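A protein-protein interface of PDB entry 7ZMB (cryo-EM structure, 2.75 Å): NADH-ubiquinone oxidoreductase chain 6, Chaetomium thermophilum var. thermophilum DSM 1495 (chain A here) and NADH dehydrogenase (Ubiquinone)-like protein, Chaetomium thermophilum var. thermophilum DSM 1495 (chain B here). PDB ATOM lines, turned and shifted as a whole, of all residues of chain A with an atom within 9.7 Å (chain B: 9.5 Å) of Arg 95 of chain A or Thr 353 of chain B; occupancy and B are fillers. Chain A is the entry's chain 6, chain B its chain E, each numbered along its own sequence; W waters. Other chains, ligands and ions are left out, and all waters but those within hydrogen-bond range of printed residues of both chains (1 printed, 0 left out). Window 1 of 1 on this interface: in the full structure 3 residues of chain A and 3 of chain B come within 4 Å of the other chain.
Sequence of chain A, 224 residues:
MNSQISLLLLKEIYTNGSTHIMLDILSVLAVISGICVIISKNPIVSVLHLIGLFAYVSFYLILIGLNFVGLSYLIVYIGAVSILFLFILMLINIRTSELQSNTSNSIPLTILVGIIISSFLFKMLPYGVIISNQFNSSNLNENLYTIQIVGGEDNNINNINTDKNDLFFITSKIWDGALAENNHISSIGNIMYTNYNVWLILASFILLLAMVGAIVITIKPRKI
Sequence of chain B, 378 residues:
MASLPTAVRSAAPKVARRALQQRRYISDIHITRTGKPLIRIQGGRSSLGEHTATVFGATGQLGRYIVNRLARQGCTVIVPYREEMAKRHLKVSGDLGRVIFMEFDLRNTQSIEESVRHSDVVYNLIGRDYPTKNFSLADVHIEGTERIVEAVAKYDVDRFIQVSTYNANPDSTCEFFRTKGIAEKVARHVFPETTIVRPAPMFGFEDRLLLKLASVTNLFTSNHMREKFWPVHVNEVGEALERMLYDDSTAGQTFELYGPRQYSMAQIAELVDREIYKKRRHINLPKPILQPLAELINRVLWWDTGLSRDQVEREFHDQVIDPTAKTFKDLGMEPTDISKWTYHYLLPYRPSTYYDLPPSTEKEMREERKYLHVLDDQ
The side-chain carboxylate of Asp 356 of chain B is in salt-bridge range of the guanidinium group of Arg 95 of chain A (3.9 Å).
The side-chain hydroxyl of Thr 353 of chain B is in hydrogen-bond range of the side-chain carboxylate of Glu 98 of chain A.
The backbone carbonyl oxygen (O) of Tyr 354 of chain B is in hydrogen-bond range of the guanidinium group (NH1) of Arg 350 of chain B (3.5 Å).
ND2 of Asn 42 of chain A sits at hydrogen-bond distance from OE2 of Glu 98 of chain A, 2.9 Å away.
The side-chain amide oxygen of Asn 93 of chain A lies close to the backbone NH of Arg 95 of chain A (3.4 Å).
Among the printed residues, pairs that only touch across the chains: Arg 95 of chain A with Thr 353 of chain B (3.8 Å), Leu 99 of chain A with Thr 353 of chain B (3.7 Å) and Leu 99 of chain A with Tyr 354 of chain B (3.6 Å).
Of chain B, only Thr 353 (3.8 Å) and Asp 356 (3.7 Å) come within 4 Å of Arg 95 of chain A.
Thr 353 of chain B touches just these residues of chain A: Arg 95, Glu 98 and Leu 99.
Thr 96 of chain A touches none of the printed residues of chain B.
Ser 97 of chain A touches none of the printed residues of chain B.
Of the printed residues of chain B, Glu 98 of chain A touches Thr 353.
Printed residues of chain A within 4 Å of Tyr 354 of chain B: Leu 99 (3.6 Å).
Printed residues of chain A within 4 Å of Asp 356 of chain B: Arg 95 (3.7 Å).
Of the printed residues of chain B, Leu 99 of chain A touches Thr 353 (3.7 Å) and Tyr 354 (3.6 Å).
Asn 93 of chain A touches none of the printed residues of chain B.
Pro 351 of chain B touches none of the printed residues of chain A.
Hydrophobic or aromatic side chains of chain A that line the printed part of chain B: Leu 99.
Of the 14 printed residues of chain B, 3 touch a printed residue of chain A.
Printed residues of chain B that touch a printed residue of chain A: Thr 353, Tyr 354 and Asp 356.
Hydrophobic or aromatic side chains of chain B that line the printed part of chain A: Tyr 354.
Among the printed residues, 5 pairs touch across the chains.
Among the printed residues, Asp or Glu carboxylates within 4 Å of a Lys or Arg side-chain nitrogen of the other chain: Arg 95 of chain A with Asp 356 of chain B (3.9 Å).
Water W1 lies within hydrogen-bond range of O of Ser 352 of chain B (2.5 Å), N of Asp 356 of chain B (3.0 Å), NH1 of Arg 95 of chain A (3.3 Å) and O of Thr 353 of chain B (3.3 Å).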
ATOM      1  N   LYS A  41      16.916  19.463  -2.645  1.00  0.00           N
ATOM      2  CA  LYS A  41      16.976  20.023  -1.301  1.00  0.00           C
ATOM      3  C   LYS A  41      18.379  20.482  -0.934  1.00  0.00           C
ATOM      4  O   LYS A  41      18.534  21.335  -0.057  1.00  0.00           O
ATOM      5  CB  LYS A  41      16.459  18.993  -0.294  1.00  0.00           C
ATOM      6  CG  LYS A  41      14.963  18.751  -0.427  1.00  0.00           C
ATOM      7  CD  LYS A  41      14.453  17.625   0.466  1.00  0.00           C
ATOM      8  CE  LYS A  41      14.462  18.001   1.934  1.00  0.00           C
ATOM      9  NZ  LYS A  41      13.853  16.929   2.769  1.00  0.00           N
ATOM     10  N   ASN A  42      19.394  19.955  -1.594  1.00  0.00           N
ATOM     11  CA  ASN A  42      20.766  20.311  -1.265  1.00  0.00           C
ATOM     12  C   ASN A  42      21.325  21.277  -2.303  1.00  0.00           C
ATOM     13  O   ASN A  42      21.223  21.012  -3.507  1.00  0.00           O
ATOM     14  CB  ASN A  42      21.627  19.055  -1.179  1.00  0.00           C
ATOM     15  CG  ASN A  42      23.096  19.358  -1.037  1.00  0.00           C
ATOM     16  OD1 ASN A  42      23.859  19.245  -1.985  1.00  0.00           O
ATOM     17  ND2 ASN A  42      23.495  19.777   0.147  1.00  0.00           N
ATOM     18  N   PRO A  43      21.888  22.416  -1.886  1.00  0.00           N
ATOM     19  CA  PRO A  43      22.349  23.422  -2.858  1.00  0.00           C
ATOM     20  C   PRO A  43      23.529  22.992  -3.703  1.00  0.00           C
ATOM     21  O   PRO A  43      23.822  23.662  -4.699  1.00  0.00           O
ATOM     22  CB  PRO A  43      22.726  24.612  -1.969  1.00  0.00           C
ATOM     23  CG  PRO A  43      21.970  24.393  -0.726  1.00  0.00           C
ATOM     24  CD  PRO A  43      21.963  22.928  -0.514  1.00  0.00           C
ATOM     25  N   ILE A  44      24.225  21.921  -3.344  1.00  0.00           N
ATOM     26  CA  ILE A  44      25.358  21.491  -4.146  1.00  0.00           C
ATOM     27  C   ILE A  44      24.945  20.510  -5.241  1.00  0.00           C
ATOM     28  O   ILE A  44      25.508  20.541  -6.340  1.00  0.00           O
ATOM     29  CB  ILE A  44      26.457  20.913  -3.242  1.00  0.00           C
ATOM     30  CG1 ILE A  44      26.882  21.959  -2.212  1.00  0.00           C
ATOM     31  CG2 ILE A  44      27.659  20.505  -4.046  1.00  0.00           C
ATOM     32  CD1 ILE A  44      27.669  23.099  -2.783  1.00  0.00           C
ATOM     33  N   ILE A  88      28.162  29.295  -2.365  1.00  0.00           N
ATOM     34  CA  ILE A  88      27.252  28.478  -1.566  1.00  0.00           C
ATOM     35  C   ILE A  88      27.938  28.000  -0.295  1.00  0.00           C
ATOM     36  O   ILE A  88      27.330  27.960   0.779  1.00  0.00           O
ATOM     37  CB  ILE A  88      26.719  27.299  -2.398  1.00  0.00           C
ATOM     38  CG1 ILE A  88      25.783  27.802  -3.495  1.00  0.00           C
ATOM     39  CG2 ILE A  88      26.006  26.306  -1.510  1.00  0.00           C
ATOM     40  CD1 ILE A  88      25.855  27.006  -4.748  1.00  0.00           C
ATOM     41  N   LEU A  89      29.214  27.634  -0.392  1.00  0.00           N
ATOM     42  CA  LEU A  89      29.946  27.175   0.784  1.00  0.00           C
ATOM     43  C   LEU A  89      30.058  28.274   1.827  1.00  0.00           C
ATOM     44  O   LEU A  89      29.935  28.018   3.027  1.00  0.00           O
ATOM     45  CB  LEU A  89      31.334  26.683   0.380  1.00  0.00           C
ATOM     46  CG  LEU A  89      31.388  25.434  -0.487  1.00  0.00           C
ATOM     47  CD1 LEU A  89      32.743  24.772  -0.394  1.00  0.00           C
ATOM     48  CD2 LEU A  89      30.295  24.484  -0.089  1.00  0.00           C
ATOM     49  N   ILE A  92      25.758  29.816   2.668  1.00  0.00           N
ATOM     50  CA  ILE A  92      24.600  28.966   2.901  1.00  0.00           C
ATOM     51  C   ILE A  92      24.982  27.924   3.935  1.00  0.00           C
ATOM     52  O   ILE A  92      26.064  27.336   3.852  1.00  0.00           O
ATOM     53  CB  ILE A  92      24.113  28.291   1.602  1.00  0.00           C
ATOM     54  CG1 ILE A  92      23.426  29.303   0.694  1.00  0.00           C
ATOM     55  CG2 ILE A  92      23.169  27.147   1.900  1.00  0.00           C
ATOM     56  CD1 ILE A  92      23.249  28.818  -0.716  1.00  0.00           C
ATOM     57  N   ASN A  93      24.117  27.721   4.920  1.00  0.00           N
ATOM     58  CA  ASN A  93      24.226  26.553   5.783  1.00  0.00           C
ATOM     59  C   ASN A  93      23.657  25.362   5.021  1.00  0.00           C
ATOM     60  O   ASN A  93      22.445  25.286   4.797  1.00  0.00           O
ATOM     61  CB  ASN A  93      23.492  26.771   7.102  1.00  0.00           C
ATOM     62  CG  ASN A  93      24.022  25.890   8.217  1.00  0.00           C
ATOM     63  OD1 ASN A  93      24.095  24.673   8.082  1.00  0.00           O
ATOM     64  ND2 ASN A  93      24.379  26.503   9.330  1.00  0.00           N
ATOM     65  N   ILE A  94      24.533  24.443   4.610  1.00  0.00           N
ATOM     66  CA  ILE A  94      24.104  23.300   3.808  1.00  0.00           C
ATOM     67  C   ILE A  94      23.114  22.439   4.575  1.00  0.00           C
ATOM     68  O   ILE A  94      22.096  22.004   4.027  1.00  0.00           O
ATOM     69  CB  ILE A  94      25.320  22.474   3.341  1.00  0.00           C
ATOM     70  CG1 ILE A  94      26.106  23.213   2.260  1.00  0.00           C
ATOM     71  CG2 ILE A  94      24.878  21.108   2.845  1.00  0.00           C
ATOM     72  CD1 ILE A  94      25.337  23.392   0.982  1.00  0.00           C
ATOM     73  N   ARG A  95      23.414  22.146   5.844  1.00  0.00           N
ATOM     74  CA  ARG A  95      22.546  21.190   6.589  1.00  0.00           C
ATOM     75  C   ARG A  95      21.152  21.783   6.794  1.00  0.00           C
ATOM     76  O   ARG A  95      20.178  21.078   6.482  1.00  0.00           O
ATOM     77  CB  ARG A  95      23.194  20.696   7.885  1.00  0.00           C
ATOM     78  CG  ARG A  95      22.621  19.379   8.388  1.00  0.00           C
ATOM     79  CD  ARG A  95      23.146  19.016   9.761  1.00  0.00           C
ATOM     80  NE  ARG A  95      22.813  20.042  10.739  1.00  0.00           N
ATOM     81  CZ  ARG A  95      23.130  19.982  12.025  1.00  0.00           C
ATOM     82  NH1 ARG A  95      23.790  18.938  12.497  1.00  0.00           N
ATOM     83  NH2 ARG A  95      22.784  20.965  12.836  1.00  0.00           N
ATOM     84  N   THR A  96      21.063  23.033   7.256  1.00  0.00           N
ATOM     85  CA  THR A  96      19.749  23.603   7.543  1.00  0.00           C
ATOM     86  C   THR A  96      18.940  23.792   6.265  1.00  0.00           C
ATOM     87  O   THR A  96      17.708  23.776   6.297  1.00  0.00           O
ATOM     88  CB  THR A  96      19.876  24.933   8.296  1.00  0.00           C
ATOM     89  OG1 THR A  96      20.575  25.887   7.498  1.00  0.00           O
ATOM     90  CG2 THR A  96      20.631  24.753   9.583  1.00  0.00           C
ATOM     91  N   SER A  97      19.616  23.965   5.130  1.00  0.00           N
ATOM     92  CA  SER A  97      18.900  24.103   3.867  1.00  0.00           C
ATOM     93  C   SER A  97      18.397  22.756   3.355  1.00  0.00           C
ATOM     94  O   SER A  97      17.334  22.682   2.734  1.00  0.00           O
ATOM     95  CB  SER A  97      19.788  24.791   2.831  1.00  0.00           C
ATOM     96  OG  SER A  97      20.635  23.872   2.188  1.00  0.00           O
ATOM     97  N   GLU A  98      19.137  21.676   3.602  1.00  0.00           N
ATOM     98  CA  GLU A  98      18.609  20.356   3.259  1.00  0.00           C
ATOM     99  C   GLU A  98      17.407  19.981   4.109  1.00  0.00           C
ATOM    100  O   GLU A  98      16.740  18.987   3.808  1.00  0.00           O
ATOM    101  CB  GLU A  98      19.677  19.278   3.411  1.00  0.00           C
ATOM    102  CG  GLU A  98      20.745  19.311   2.363  1.00  0.00           C
ATOM    103  CD  GLU A  98      21.843  18.309   2.637  1.00  0.00           C
ATOM    104  OE1 GLU A  98      22.279  18.208   3.805  1.00  0.00           O
ATOM    105  OE2 GLU A  98      22.263  17.613   1.688  1.00  0.00           O
ATOM    106  N   LEU A  99      17.147  20.732   5.172  1.00  0.00           N
ATOM    107  CA  LEU A  99      15.949  20.607   5.982  1.00  0.00           C
ATOM    108  C   LEU A  99      14.906  21.650   5.614  1.00  0.00           C
ATOM    109  O   LEU A  99      13.839  21.698   6.230  1.00  0.00           O
ATOM    110  CB  LEU A  99      16.329  20.728   7.457  1.00  0.00           C
ATOM    111  CG  LEU A  99      17.333  19.648   7.827  1.00  0.00           C
ATOM    112  CD1 LEU A  99      18.143  20.000   9.056  1.00  0.00           C
ATOM    113  CD2 LEU A  99      16.526  18.417   8.055  1.00  0.00           C
ATOM    114  N   GLN A 100      15.199  22.482   4.618  1.00  0.00           N
ATOM    115  CA  GLN A 100      14.334  23.582   4.205  1.00  0.00           C
ATOM    116  C   GLN A 100      13.239  23.067   3.267  1.00  0.00           C
ATOM    117  O   GLN A 100      13.108  23.479   2.114  1.00  0.00           O
ATOM    118  CB  GLN A 100      15.188  24.657   3.546  1.00  0.00           C
ATOM    119  CG  GLN A 100      14.672  26.078   3.603  1.00  0.00           C
ATOM    120  CD  GLN A 100      15.547  27.011   2.788  1.00  0.00           C
ATOM    121  OE1 GLN A 100      16.475  26.567   2.118  1.00  0.00           O
ATOM    122  NE2 GLN A 100      15.262  28.302   2.848  1.00  0.00           N
ATOM    123  N   SER A 101      12.444  22.136   3.792  1.00  0.00           N
ATOM    124  CA  SER A 101      11.452  21.449   2.978  1.00  0.00           C
ATOM    125  C   SER A 101      10.359  22.407   2.525  1.00  0.00           C
ATOM    126  O   SER A 101       9.972  23.327   3.251  1.00  0.00           O
ATOM    127  CB  SER A 101      10.841  20.284   3.759  1.00  0.00           C
ATOM    128  OG  SER A 101      10.168  20.740   4.918  1.00  0.00           O
ATOM    129  N   GLU B 275      15.180   4.883  12.404  1.00  0.00           N
ATOM    130  CA  GLU B 275      16.489   5.143  12.980  1.00  0.00           C
ATOM    131  C   GLU B 275      17.460   5.721  11.961  1.00  0.00           C
ATOM    132  O   GLU B 275      18.083   6.754  12.212  1.00  0.00           O
ATOM    133  CB  GLU B 275      17.045   3.855  13.586  1.00  0.00           C
ATOM    134  CG  GLU B 275      18.086   4.065  14.662  1.00  0.00           C
ATOM    135  CD  GLU B 275      17.647   5.029  15.737  1.00  0.00           C
ATOM    136  OE1 GLU B 275      17.005   4.583  16.709  1.00  0.00           O
ATOM    137  OE2 GLU B 275      17.963   6.231  15.627  1.00  0.00           O
ATOM    138  N   ILE B 276      17.584   5.082  10.800  1.00  0.00           N
ATOM    139  CA  ILE B 276      18.495   5.583   9.783  1.00  0.00           C
ATOM    140  C   ILE B 276      17.910   6.766   9.026  1.00  0.00           C
ATOM    141  O   ILE B 276      18.658   7.492   8.366  1.00  0.00           O
ATOM    142  CB  ILE B 276      18.886   4.469   8.798  1.00  0.00           C
ATOM    143  CG1 ILE B 276      17.673   4.003   7.992  1.00  0.00           C
ATOM    144  CG2 ILE B 276      19.510   3.300   9.540  1.00  0.00           C
ATOM    145  CD1 ILE B 276      17.958   2.834   7.081  1.00  0.00           C
ATOM    146  N   TYR B 277      16.599   6.978   9.108  1.00  0.00           N
ATOM    147  CA  TYR B 277      15.920   8.078   8.424  1.00  0.00           C
ATOM    148  C   TYR B 277      16.032   7.937   6.907  1.00  0.00           C
ATOM    149  O   TYR B 277      16.354   8.892   6.200  1.00  0.00           O
ATOM    150  CB  TYR B 277      16.470   9.442   8.862  1.00  0.00           C
ATOM    151  CG  TYR B 277      15.998   9.975  10.196  1.00  0.00           C
ATOM    152  CD1 TYR B 277      14.872  10.770  10.286  1.00  0.00           C
ATOM    153  CD2 TYR B 277      16.726   9.739  11.356  1.00  0.00           C
ATOM    154  CE1 TYR B 277      14.451  11.271  11.501  1.00  0.00           C
ATOM    155  CE2 TYR B 277      16.317  10.231  12.567  1.00  0.00           C
ATOM    156  CZ  TYR B 277      15.179  10.999  12.637  1.00  0.00           C
ATOM    157  OH  TYR B 277      14.764  11.502  13.850  1.00  0.00           O
ATOM    158  N   LYS B 278      15.761   6.735   6.398  1.00  0.00           N
ATOM    159  CA  LYS B 278      16.031   6.482   4.986  1.00  0.00           C
ATOM    160  C   LYS B 278      14.832   5.942   4.217  1.00  0.00           C
ATOM    161  O   LYS B 278      14.732   6.158   3.004  1.00  0.00           O
ATOM    162  CB  LYS B 278      17.207   5.514   4.835  1.00  0.00           C
ATOM    163  CG  LYS B 278      18.563   6.121   5.130  1.00  0.00           C
ATOM    164  CD  LYS B 278      19.147   6.769   3.889  1.00  0.00           C
ATOM    165  CE  LYS B 278      20.481   7.443   4.176  1.00  0.00           C
ATOM    166  NZ  LYS B 278      21.538   6.479   4.580  1.00  0.00           N
ATOM    167  N   TYR B 349      24.584   4.294   9.583  1.00  0.00           N
ATOM    168  CA  TYR B 349      23.819   4.327   8.348  1.00  0.00           C
ATOM    169  C   TYR B 349      22.879   5.517   8.273  1.00  0.00           C
ATOM    170  O   TYR B 349      22.059   5.589   7.356  1.00  0.00           O
ATOM    171  CB  TYR B 349      23.058   3.009   8.162  1.00  0.00           C
ATOM    172  CG  TYR B 349      23.954   1.788   8.199  1.00  0.00           C
ATOM    173  CD1 TYR B 349      24.585   1.395   9.369  1.00  0.00           C
ATOM    174  CD2 TYR B 349      24.185   1.043   7.055  1.00  0.00           C
ATOM    175  CE1 TYR B 349      25.411   0.299   9.405  1.00  0.00           C
ATOM    176  CE2 TYR B 349      25.011  -0.067   7.082  1.00  0.00           C
ATOM    177  CZ  TYR B 349      25.622  -0.429   8.263  1.00  0.00           C
ATOM    178  OH  TYR B 349      26.446  -1.526   8.302  1.00  0.00           O
ATOM    179  N   ARG B 350      22.980   6.420   9.232  1.00  0.00           N
ATOM    180  CA  ARG B 350      22.168   7.658   9.146  1.00  0.00           C
ATOM    181  C   ARG B 350      22.830   8.592   8.139  1.00  0.00           C
ATOM    182  O   ARG B 350      24.067   8.669   8.141  1.00  0.00           O
ATOM    183  CB  ARG B 350      22.069   8.373  10.497  1.00  0.00           C
ATOM    184  CG  ARG B 350      21.099   7.746  11.483  1.00  0.00           C
ATOM    185  CD  ARG B 350      21.051   8.632  12.707  1.00  0.00           C
ATOM    186  NE  ARG B 350      19.815   8.520  13.458  1.00  0.00           N
ATOM    187  CZ  ARG B 350      19.582   9.158  14.596  1.00  0.00           C
ATOM    188  NH1 ARG B 350      20.511   9.943  15.107  1.00  0.00           N
ATOM    189  NH2 ARG B 350      18.429   9.003  15.219  1.00  0.00           N
ATOM    190  N   PRO B 351      22.068   9.322   7.299  1.00  0.00           N
ATOM    191  CA  PRO B 351      22.654  10.299   6.396  1.00  0.00           C
ATOM    192  C   PRO B 351      23.204  11.451   7.242  1.00  0.00           C
ATOM    193  O   PRO B 351      22.717  11.661   8.329  1.00  0.00           O
ATOM    194  CB  PRO B 351      21.489  10.747   5.510  1.00  0.00           C
ATOM    195  CG  PRO B 351      20.268  10.502   6.357  1.00  0.00           C
ATOM    196  CD  PRO B 351      20.613   9.300   7.208  1.00  0.00           C
ATOM    197  N   SER B 352      24.215  12.142   6.736  1.00  0.00           N
ATOM    198  CA  SER B 352      24.853  13.273   7.455  1.00  0.00           C
ATOM    199  C   SER B 352      23.834  14.260   8.039  1.00  0.00           C
ATOM    200  O   SER B 352      24.084  14.744   9.147  1.00  0.00           O
ATOM    201  CB  SER B 352      25.784  13.958   6.515  1.00  0.00           C
ATOM    202  OG  SER B 352      25.077  14.464   5.397  1.00  0.00           O
ATOM    203  N   THR B 353      22.761  14.583   7.313  1.00  0.00           N
ATOM    204  CA  THR B 353      21.767  15.591   7.763  1.00  0.00           C
ATOM    205  C   THR B 353      21.134  15.149   9.075  1.00  0.00           C
ATOM    206  O   THR B 353      20.891  16.011   9.935  1.00  0.00           O
ATOM    207  CB  THR B 353      20.674  15.783   6.703  1.00  0.00           C
ATOM    208  OG1 THR B 353      21.312  15.919   5.433  1.00  0.00           O
ATOM    209  CG2 THR B 353      19.791  16.980   6.966  1.00  0.00           C
ATOM    210  N   TYR B 354      20.861  13.858   9.218  1.00  0.00           N
ATOM    211  CA  TYR B 354      20.137  13.393  10.429  1.00  0.00           C
ATOM    212  C   TYR B 354      21.077  12.698  11.406  1.00  0.00           C
ATOM    213  O   TYR B 354      20.590  12.172  12.410  1.00  0.00           O
ATOM    214  CB  TYR B 354      18.941  12.539  10.005  1.00  0.00           C
ATOM    215  CG  TYR B 354      18.071  13.201   8.972  1.00  0.00           C
ATOM    216  CD1 TYR B 354      17.165  14.184   9.329  1.00  0.00           C
ATOM    217  CD2 TYR B 354      18.163  12.860   7.633  1.00  0.00           C
ATOM    218  CE1 TYR B 354      16.365  14.803   8.384  1.00  0.00           C
ATOM    219  CE2 TYR B 354      17.373  13.469   6.675  1.00  0.00           C
ATOM    220  CZ  TYR B 354      16.468  14.444   7.052  1.00  0.00           C
ATOM    221  OH  TYR B 354      15.683  15.051   6.115  1.00  0.00           O
ATOM    222  N   TYR B 355      22.375  12.663  11.111  1.00  0.00           N
ATOM    223  CA  TYR B 355      23.318  11.897  11.966  1.00  0.00           C
ATOM    224  C   TYR B 355      23.418  12.481  13.382  1.00  0.00           C
ATOM    225  O   TYR B 355      23.394  11.684  14.333  1.00  0.00           O
ATOM    226  CB  TYR B 355      24.682  11.831  11.277  1.00  0.00           C
ATOM    227  CG  TYR B 355      25.697  10.937  11.946  1.00  0.00           C
ATOM    228  CD1 TYR B 355      26.469  11.393  13.001  1.00  0.00           C
ATOM    229  CD2 TYR B 355      25.889   9.636  11.516  1.00  0.00           C
ATOM    230  CE1 TYR B 355      27.393  10.573  13.626  1.00  0.00           C
ATOM    231  CE2 TYR B 355      26.818   8.807  12.121  1.00  0.00           C
ATOM    232  CZ  TYR B 355      27.570   9.276  13.181  1.00  0.00           C
ATOM    233  OH  TYR B 355      28.483   8.462  13.784  1.00  0.00           O
ATOM    234  N   ASP B 356      23.502  13.805  13.527  1.00  0.00           N
ATOM    235  CA  ASP B 356      23.737  14.449  14.849  1.00  0.00           C
ATOM    236  C   ASP B 356      22.510  14.383  15.752  1.00  0.00           C
ATOM    237  O   ASP B 356      22.592  14.882  16.874  1.00  0.00           O
ATOM    238  CB  ASP B 356      24.128  15.917  14.686  1.00  0.00           C
ATOM    239  CG  ASP B 356      25.116  16.395  15.737  1.00  0.00           C
ATOM    240  OD1 ASP B 356      25.590  15.549  16.524  1.00  0.00           O
ATOM    241  OD2 ASP B 356      25.402  17.609  15.762  1.00  0.00           O
ATOM    242  N   LEU B 357      21.419  13.804  15.272  1.00  0.00           N
ATOM    243  CA  LEU B 357      20.205  13.730  16.058  1.00  0.00           C
ATOM    244  C   LEU B 357      20.289  12.686  17.168  1.00  0.00           C
ATOM    245  O   LEU B 357      21.085  11.748  17.100  1.00  0.00           O
ATOM    246  CB  LEU B 357      19.033  13.444  15.127  1.00  0.00           C
ATOM    247  CG  LEU B 357      18.531  14.661  14.355  1.00  0.00           C
ATOM    248  CD1 LEU B 357      19.482  15.123  13.294  1.00  0.00           C
ATOM    249  CD2 LEU B 357      17.224  14.263  13.706  1.00  0.00           C
ATOM    250  N   PRO B 358      19.474  12.840  18.210  1.00  0.00           N
ATOM    251  CA  PRO B 358      19.479  11.880  19.315  1.00  0.00           C
ATOM    252  C   PRO B 358      18.792  10.589  18.913  1.00  0.00           C
ATOM    253  O   PRO B 358      18.174  10.517  17.842  1.00  0.00           O
ATOM    254  CB  PRO B 358      18.698  12.611  20.424  1.00  0.00           C
ATOM    255  CG  PRO B 358      18.564  14.012  19.969  1.00  0.00           C
ATOM    256  CD  PRO B 358      18.580  13.972  18.490  1.00  0.00           C
HETATM  257  O   HOH W   1      23.827  15.843  11.403  1.00  0.00           O
